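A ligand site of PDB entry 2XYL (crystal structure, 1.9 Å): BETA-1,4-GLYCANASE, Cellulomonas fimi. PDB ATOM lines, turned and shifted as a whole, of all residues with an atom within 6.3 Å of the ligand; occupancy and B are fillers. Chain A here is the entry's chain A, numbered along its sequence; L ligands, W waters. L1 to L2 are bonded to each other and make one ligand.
The side-chain amide nitrogen of Asn 126 lies close to a fluorine (F1) of LIG L1, 3.3 Å away. Residues that only touch the ligand: Trp 84 (3.3 Å), Glu 127 (3.9 Å), Gln 203 (3.3 Å) and Trp 281 (3.6 Å). Hydrophobic or aromatic side chains that line the ligand: His 80, Trp 84, His 205, Trp 273 and Trp 281. Of the 18 residues printed, 13 come within 4 Å of the ligand.
O of Gln 203 lies close to N of Glu 233, at 2.9 Å. The side-chain amide oxygen (OD1) of Asn 44 lies within hydrogen-bond range of the side-chain amino group (NZ) of Lys 47 (2.8 Å). The side-chain amide oxygen of Gln 87 lies close to the side-chain amide oxygen of Asn 44 (3.5 Å). NE2 of His 205 lies close to OE1 of Gln 203, 3.5 Å away. The side-chain carboxylate (OE2) of Glu 127 lies within hydrogen-bond range of the side-chain amide nitrogen (ND2) of Asn 126, 3.5 Å away. The side-chain amide nitrogen (ND2) of Asn 169 sits at hydrogen-bond distance from the side-chain amide oxygen (OD1) of Asn 126 (2.8 Å). NE2 of Gln 203 is in hydrogen-bond range of OE2 of Glu 127, 2.8 Å away. The backbone NH (N) of Glu 127 is in hydrogen-bond range of the backbone carbonyl oxygen (O) of Asn 169.
The side-chain carboxylate (OE1) of Glu 233 is covalently linked to a carbon (C1) of LIG L1 (1.4 Å). An oxygen (O1) of LIG L1 is in hydrogen-bond range of the side-chain amino group of Lys 47, at 2.8 Å. An oxygen (O1) of LG2 L2 sits at hydrogen-bond distance from the indole nitrogen (NE1) of Trp 273, at 2.9 Å. The side-chain carboxylate (OE2) of Glu 43 lies within hydrogen-bond range of an oxygen (O1) of LG2 L2, at 2.9 Å. The side-chain amide nitrogen (ND2) of Asn 44 is in hydrogen-bond range of an oxygen (O2) of LG2 L2 (3.0 Å). An oxygen (O1) of LIG L1 lies within hydrogen-bond range of a ring nitrogen (NE2) of His 80 (3.0 Å). An oxygen (O3) of LIG L1 lies within hydrogen-bond range of a ring nitrogen (NE2) of His 205, at 3.0 Å. NE2 of Gln 87 sits close to O4 of LG2 L2 (3.4 Å).
Water W2 bridges OE2 of Glu 127 (2.9 Å) and O3 of LIG L1 (3.1 Å). Water W3 bridges NE2 of Gln 87 (2.8 Å) and OG of Ser 86 (2.9 Å).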
ATOM      1  N   GLU A  43      14.677  23.757 -18.874  1.00  0.00           N
ATOM      2  CA  GLU A  43      14.584  23.969 -17.437  1.00  0.00           C
ATOM      3  C   GLU A  43      14.367  22.632 -16.725  1.00  0.00           C
ATOM      4  O   GLU A  43      14.938  22.392 -15.656  1.00  0.00           O
ATOM      5  CB  GLU A  43      13.438  24.934 -17.087  1.00  0.00           C
ATOM      6  CG  GLU A  43      13.331  25.245 -15.594  1.00  0.00           C
ATOM      7  CD  GLU A  43      12.118  26.098 -15.229  1.00  0.00           C
ATOM      8  OE1 GLU A  43      11.073  26.002 -15.916  1.00  0.00           O
ATOM      9  OE2 GLU A  43      12.199  26.848 -14.229  1.00  0.00           O
ATOM     10  N   ASN A  44      13.581  21.756 -17.338  1.00  0.00           N
ATOM     11  CA  ASN A  44      13.285  20.451 -16.748  1.00  0.00           C
ATOM     12  C   ASN A  44      13.135  19.328 -17.761  1.00  0.00           C
ATOM     13  O   ASN A  44      13.315  18.162 -17.422  1.00  0.00           O
ATOM     14  CB  ASN A  44      11.989  20.518 -15.917  1.00  0.00           C
ATOM     15  CG  ASN A  44      12.129  21.378 -14.680  1.00  0.00           C
ATOM     16  OD1 ASN A  44      12.774  20.994 -13.702  1.00  0.00           O
ATOM     17  ND2 ASN A  44      11.515  22.551 -14.703  1.00  0.00           N
ATOM     18  N   LYS A  47      15.896  16.355 -17.952  1.00  0.00           N
ATOM     19  CA  LYS A  47      16.344  15.688 -16.734  1.00  0.00           C
ATOM     20  C   LYS A  47      15.966  14.204 -16.732  1.00  0.00           C
ATOM     21  O   LYS A  47      15.211  13.743 -17.596  1.00  0.00           O
ATOM     22  CB  LYS A  47      15.791  16.400 -15.489  1.00  0.00           C
ATOM     23  CG  LYS A  47      16.362  17.795 -15.300  1.00  0.00           C
ATOM     24  CD  LYS A  47      15.682  18.568 -14.186  1.00  0.00           C
ATOM     25  CE  LYS A  47      16.283  19.957 -14.065  1.00  0.00           C
ATOM     26  NZ  LYS A  47      15.527  20.832 -13.127  1.00  0.00           N
ATOM     27  N   HIS A  80      20.904  19.951 -20.374  1.00  0.00           N
ATOM     28  CA  HIS A  80      20.934  20.017 -18.925  1.00  0.00           C
ATOM     29  C   HIS A  80      20.825  18.700 -18.165  1.00  0.00           C
ATOM     30  O   HIS A  80      19.795  18.036 -18.150  1.00  0.00           O
ATOM     31  CB  HIS A  80      19.929  21.026 -18.379  1.00  0.00           C
ATOM     32  CG  HIS A  80      20.056  21.258 -16.906  1.00  0.00           C
ATOM     33  ND1 HIS A  80      21.277  21.427 -16.292  1.00  0.00           N
ATOM     34  CD2 HIS A  80      19.130  21.298 -15.921  1.00  0.00           C
ATOM     35  CE1 HIS A  80      21.094  21.570 -14.988  1.00  0.00           C
ATOM     36  NE2 HIS A  80      19.802  21.500 -14.737  1.00  0.00           N
ATOM     37  N   THR A  81      21.947  18.408 -17.526  1.00  0.00           N
ATOM     38  CA  THR A  81      22.209  17.241 -16.695  1.00  0.00           C
ATOM     39  C   THR A  81      21.719  15.825 -16.990  1.00  0.00           C
ATOM     40  O   THR A  81      20.519  15.536 -17.031  1.00  0.00           O
ATOM     41  CB  THR A  81      22.029  17.577 -15.211  1.00  0.00           C
ATOM     42  OG1 THR A  81      22.811  16.675 -14.427  1.00  0.00           O
ATOM     43  CG2 THR A  81      20.564  17.497 -14.795  1.00  0.00           C
ATOM     44  N   TRP A  84      22.303  13.467 -11.861  1.00  0.00           N
ATOM     45  CA  TRP A  84      21.967  14.405 -10.793  1.00  0.00           C
ATOM     46  C   TRP A  84      21.196  13.672  -9.703  1.00  0.00           C
ATOM     47  O   TRP A  84      20.284  12.900  -9.999  1.00  0.00           O
ATOM     48  CB  TRP A  84      21.116  15.539 -11.366  1.00  0.00           C
ATOM     49  CG  TRP A  84      20.903  16.694 -10.444  1.00  0.00           C
ATOM     50  CD1 TRP A  84      21.744  17.127  -9.463  1.00  0.00           C
ATOM     51  CD2 TRP A  84      19.793  17.605 -10.442  1.00  0.00           C
ATOM     52  NE1 TRP A  84      21.221  18.237  -8.845  1.00  0.00           N
ATOM     53  CE2 TRP A  84      20.024  18.555  -9.426  1.00  0.00           C
ATOM     54  CE3 TRP A  84      18.615  17.697 -11.204  1.00  0.00           C
ATOM     55  CZ2 TRP A  84      19.131  19.594  -9.148  1.00  0.00           C
ATOM     56  CZ3 TRP A  84      17.728  18.727 -10.926  1.00  0.00           C
ATOM     57  CH2 TRP A  84      17.986  19.658  -9.905  1.00  0.00           C
ATOM     58  N   SER A  86      19.097  14.921  -7.585  1.00  0.00           N
ATOM     59  CA  SER A  86      17.722  15.422  -7.480  1.00  0.00           C
ATOM     60  C   SER A  86      16.928  15.072  -8.740  1.00  0.00           C
ATOM     61  O   SER A  86      17.497  14.867  -9.808  1.00  0.00           O
ATOM     62  CB  SER A  86      17.725  16.935  -7.242  1.00  0.00           C
ATOM     63  OG  SER A  86      16.423  17.413  -6.949  1.00  0.00           O
ATOM     64  N   GLN A  87      15.604  15.016  -8.591  1.00  0.00           N
ATOM     65  CA  GLN A  87      14.697  14.670  -9.681  1.00  0.00           C
ATOM     66  C   GLN A  87      15.089  13.348 -10.341  1.00  0.00           C
ATOM     67  O   GLN A  87      15.187  13.248 -11.565  1.00  0.00           O
ATOM     68  CB  GLN A  87      14.588  15.810 -10.703  1.00  0.00           C
ATOM     69  CG  GLN A  87      13.729  16.957 -10.212  1.00  0.00           C
ATOM     70  CD  GLN A  87      13.538  18.034 -11.261  1.00  0.00           C
ATOM     71  OE1 GLN A  87      12.695  17.908 -12.148  1.00  0.00           O
ATOM     72  NE2 GLN A  87      14.301  19.112 -11.144  1.00  0.00           N
ATOM     73  N   ASP A 123      25.677  18.935 -19.248  1.00  0.00           N
ATOM     74  CA  ASP A 123      25.984  18.995 -17.825  1.00  0.00           C
ATOM     75  C   ASP A 123      25.989  17.508 -17.514  1.00  0.00           C
ATOM     76  O   ASP A 123      24.943  16.932 -17.236  1.00  0.00           O
ATOM     77  CB  ASP A 123      24.869  19.693 -17.034  1.00  0.00           C
ATOM     78  CG  ASP A 123      25.052  21.186 -16.933  1.00  0.00           C
ATOM     79  OD1 ASP A 123      26.179  21.684 -17.133  1.00  0.00           O
ATOM     80  OD2 ASP A 123      24.058  21.880 -16.629  1.00  0.00           O
ATOM     81  N   ASN A 126      25.962  17.022 -12.234  1.00  0.00           N
ATOM     82  CA  ASN A 126      25.488  18.245 -11.613  1.00  0.00           C
ATOM     83  C   ASN A 126      25.427  18.102 -10.090  1.00  0.00           C
ATOM     84  O   ASN A 126      24.934  17.096  -9.568  1.00  0.00           O
ATOM     85  CB  ASN A 126      24.092  18.580 -12.159  1.00  0.00           C
ATOM     86  CG  ASN A 126      23.577  19.928 -11.701  1.00  0.00           C
ATOM     87  OD1 ASN A 126      24.228  20.954 -11.914  1.00  0.00           O
ATOM     88  ND2 ASN A 126      22.388  19.939 -11.124  1.00  0.00           N
ATOM     89  N   GLU A 127      26.010  19.076  -9.386  1.00  0.00           N
ATOM     90  CA  GLU A 127      26.017  19.128  -7.925  1.00  0.00           C
ATOM     91  C   GLU A 127      26.538  17.873  -7.212  1.00  0.00           C
ATOM     92  O   GLU A 127      25.842  17.289  -6.374  1.00  0.00           O
ATOM     93  CB  GLU A 127      24.615  19.489  -7.433  1.00  0.00           C
ATOM     94  CG  GLU A 127      24.101  20.784  -8.048  1.00  0.00           C
ATOM     95  CD  GLU A 127      22.649  21.063  -7.748  1.00  0.00           C
ATOM     96  OE1 GLU A 127      22.044  20.359  -6.904  1.00  0.00           O
ATOM     97  OE2 GLU A 127      22.105  21.999  -8.362  1.00  0.00           O
ATOM     98  N   ASN A 169      28.751  20.706 -13.430  1.00  0.00           N
ATOM     99  CA  ASN A 169      28.045  21.888 -12.934  1.00  0.00           C
ATOM    100  C   ASN A 169      27.842  21.880 -11.423  1.00  0.00           C
ATOM    101  O   ASN A 169      27.693  20.820 -10.818  1.00  0.00           O
ATOM    102  CB  ASN A 169      26.699  21.970 -13.655  1.00  0.00           C
ATOM    103  CG  ASN A 169      26.070  23.346 -13.583  1.00  0.00           C
ATOM    104  OD1 ASN A 169      26.731  24.355 -13.796  1.00  0.00           O
ATOM    105  ND2 ASN A 169      24.773  23.392 -13.284  1.00  0.00           N
ATOM    106  N   GLN A 203      26.699  27.754 -11.424  1.00  0.00           N
ATOM    107  CA  GLN A 203      25.287  28.078 -11.321  1.00  0.00           C
ATOM    108  C   GLN A 203      24.985  29.554 -11.101  1.00  0.00           C
ATOM    109  O   GLN A 203      24.208  30.154 -11.837  1.00  0.00           O
ATOM    110  CB  GLN A 203      24.604  27.211 -10.265  1.00  0.00           C
ATOM    111  CG  GLN A 203      24.572  25.736 -10.647  1.00  0.00           C
ATOM    112  CD  GLN A 203      23.656  24.896  -9.780  1.00  0.00           C
ATOM    113  OE1 GLN A 203      22.797  25.410  -9.079  1.00  0.00           O
ATOM    114  NE2 GLN A 203      23.843  23.587  -9.841  1.00  0.00           N
ATOM    115  N   HIS A 205      23.520  31.137  -8.369  1.00  0.00           N
ATOM    116  CA  HIS A 205      22.231  31.428  -7.738  1.00  0.00           C
ATOM    117  C   HIS A 205      22.608  32.330  -6.568  1.00  0.00           C
ATOM    118  O   HIS A 205      22.746  31.880  -5.426  1.00  0.00           O
ATOM    119  CB  HIS A 205      21.544  30.149  -7.248  1.00  0.00           C
ATOM    120  CG  HIS A 205      20.937  29.329  -8.344  1.00  0.00           C
ATOM    121  ND1 HIS A 205      19.930  29.797  -9.159  1.00  0.00           N
ATOM    122  CD2 HIS A 205      21.194  28.057  -8.759  1.00  0.00           C
ATOM    123  CE1 HIS A 205      19.587  28.851 -10.028  1.00  0.00           C
ATOM    124  NE2 HIS A 205      20.342  27.793  -9.805  1.00  0.00           N
ATOM    125  N   GLU A 233      23.195  29.060 -14.343  1.00  0.00           N
ATOM    126  CA  GLU A 233      21.832  29.291 -13.877  1.00  0.00           C
ATOM    127  C   GLU A 233      21.672  30.570 -13.090  1.00  0.00           C
ATOM    128  O   GLU A 233      21.109  30.579 -11.992  1.00  0.00           O
ATOM    129  CB  GLU A 233      21.414  28.090 -13.030  1.00  0.00           C
ATOM    130  CG  GLU A 233      21.787  26.758 -13.623  1.00  0.00           C
ATOM    131  CD  GLU A 233      21.455  25.589 -12.708  1.00  0.00           C
ATOM    132  OE1 GLU A 233      20.213  25.593 -11.984  1.00  0.00           O
ATOM    133  OE2 GLU A 233      22.278  24.665 -12.630  1.00  0.00           O
ATOM    134  N   TRP A 273      18.509  31.722 -15.394  1.00  0.00           N
ATOM    135  CA  TRP A 273      17.540  30.675 -15.141  1.00  0.00           C
ATOM    136  C   TRP A 273      16.078  31.118 -15.286  1.00  0.00           C
ATOM    137  O   TRP A 273      15.317  31.131 -14.318  1.00  0.00           O
ATOM    138  CB  TRP A 273      17.790  30.005 -13.793  1.00  0.00           C
ATOM    139  CG  TRP A 273      17.361  28.571 -13.784  1.00  0.00           C
ATOM    140  CD1 TRP A 273      16.406  28.013 -12.979  1.00  0.00           C
ATOM    141  CD2 TRP A 273      17.825  27.539 -14.644  1.00  0.00           C
ATOM    142  NE1 TRP A 273      16.242  26.681 -13.300  1.00  0.00           N
ATOM    143  CE2 TRP A 273      17.107  26.367 -14.317  1.00  0.00           C
ATOM    144  CE3 TRP A 273      18.778  27.479 -15.669  1.00  0.00           C
ATOM    145  CZ2 TRP A 273      17.311  25.152 -14.984  1.00  0.00           C
ATOM    146  CZ3 TRP A 273      18.986  26.267 -16.327  1.00  0.00           C
ATOM    147  CH2 TRP A 273      18.252  25.121 -15.978  1.00  0.00           C
ATOM    148  N   TRP A 281      11.718  29.991 -10.374  1.00  0.00           N
ATOM    149  CA  TRP A 281      11.651  28.905  -9.393  1.00  0.00           C
ATOM    150  C   TRP A 281      11.963  29.346  -7.967  1.00  0.00           C
ATOM    151  O   TRP A 281      11.638  28.641  -7.006  1.00  0.00           O
ATOM    152  CB  TRP A 281      12.629  27.787  -9.786  1.00  0.00           C
ATOM    153  CG  TRP A 281      14.084  28.109  -9.459  1.00  0.00           C
ATOM    154  CD1 TRP A 281      14.785  29.223  -9.830  1.00  0.00           C
ATOM    155  CD2 TRP A 281      14.979  27.313  -8.662  1.00  0.00           C
ATOM    156  NE1 TRP A 281      16.056  29.174  -9.311  1.00  0.00           N
ATOM    157  CE2 TRP A 281      16.201  28.015  -8.601  1.00  0.00           C
ATOM    158  CE3 TRP A 281      14.866  26.086  -8.015  1.00  0.00           C
ATOM    159  CZ2 TRP A 281      17.302  27.522  -7.897  1.00  0.00           C
ATOM    160  CZ3 TRP A 281      15.966  25.593  -7.311  1.00  0.00           C
ATOM    161  CH2 TRP A 281      17.169  26.319  -7.259  1.00  0.00           C
ATOM    162  N   VAL A 285      11.291  27.653  -3.715  1.00  0.00           N
ATOM    163  CA  VAL A 285      12.414  27.056  -3.014  1.00  0.00           C
ATOM    164  C   VAL A 285      12.897  27.940  -1.862  1.00  0.00           C
ATOM    165  O   VAL A 285      13.181  27.451  -0.780  1.00  0.00           O
ATOM    166  CB  VAL A 285      13.596  26.798  -3.990  1.00  0.00           C
ATOM    167  CG1 VAL A 285      14.805  26.266  -3.254  1.00  0.00           C
ATOM    168  CG2 VAL A 285      13.171  25.821  -5.074  1.00  0.00           C
HETATM  169  C1  LIG L   1      20.132  24.700 -10.871  1.00  0.00           C
HETATM  170  C2  LIG L   1      19.770  23.255 -11.313  1.00  0.00           C
HETATM  171  C3  LIG L   1      18.426  23.208 -12.055  1.00  0.00           C
HETATM  172  C4  LIG L   1      17.370  23.813 -11.150  1.00  0.00           C
HETATM  173  C5  LIG L   1      17.839  25.196 -10.703  1.00  0.00           C
HETATM  174  O1  LIG L   1      18.062  21.869 -12.368  1.00  0.00           O
HETATM  175  O2  LIG L   1      16.136  23.953 -11.867  1.00  0.00           O
HETATM  176  O3  LIG L   1      19.077  25.083  -9.995  1.00  0.00           O
HETATM  177  F1  LIG L   1      20.810  22.654 -12.021  1.00  0.00           F
HETATM  178  C1  LG2 L   2      14.989  23.746 -11.112  1.00  0.00           C
HETATM  179  C2  LG2 L   2      13.770  24.140 -11.940  1.00  0.00           C
HETATM  180  C3  LG2 L   2      12.456  23.828 -11.243  1.00  0.00           C
HETATM  181  C4  LG2 L   2      12.464  22.380 -10.798  1.00  0.00           C
HETATM  182  C5  LG2 L   2      13.676  22.099  -9.931  1.00  0.00           C
HETATM  183  O1  LG2 L   2      13.840  25.498 -12.259  1.00  0.00           O
HETATM  184  O2  LG2 L   2      11.402  24.041 -12.157  1.00  0.00           O
HETATM  185  O3  LG2 L   2      11.290  22.097 -10.055  1.00  0.00           O
HETATM  186  O4  LG2 L   2      14.880  22.401 -10.669  1.00  0.00           O
HETATM  187  O   HOH W   1      11.310  23.763  -7.547  1.00  0.00           O
HETATM  188  O   HOH W   2      19.444  22.980  -7.714  1.00  0.00           O
HETATM  189  O   HOH W   3      14.985  19.440  -8.409  1.00  0.00           O
HETATM  190  O   HOH W   4       9.788  25.970 -10.669  1.00  0.00           O
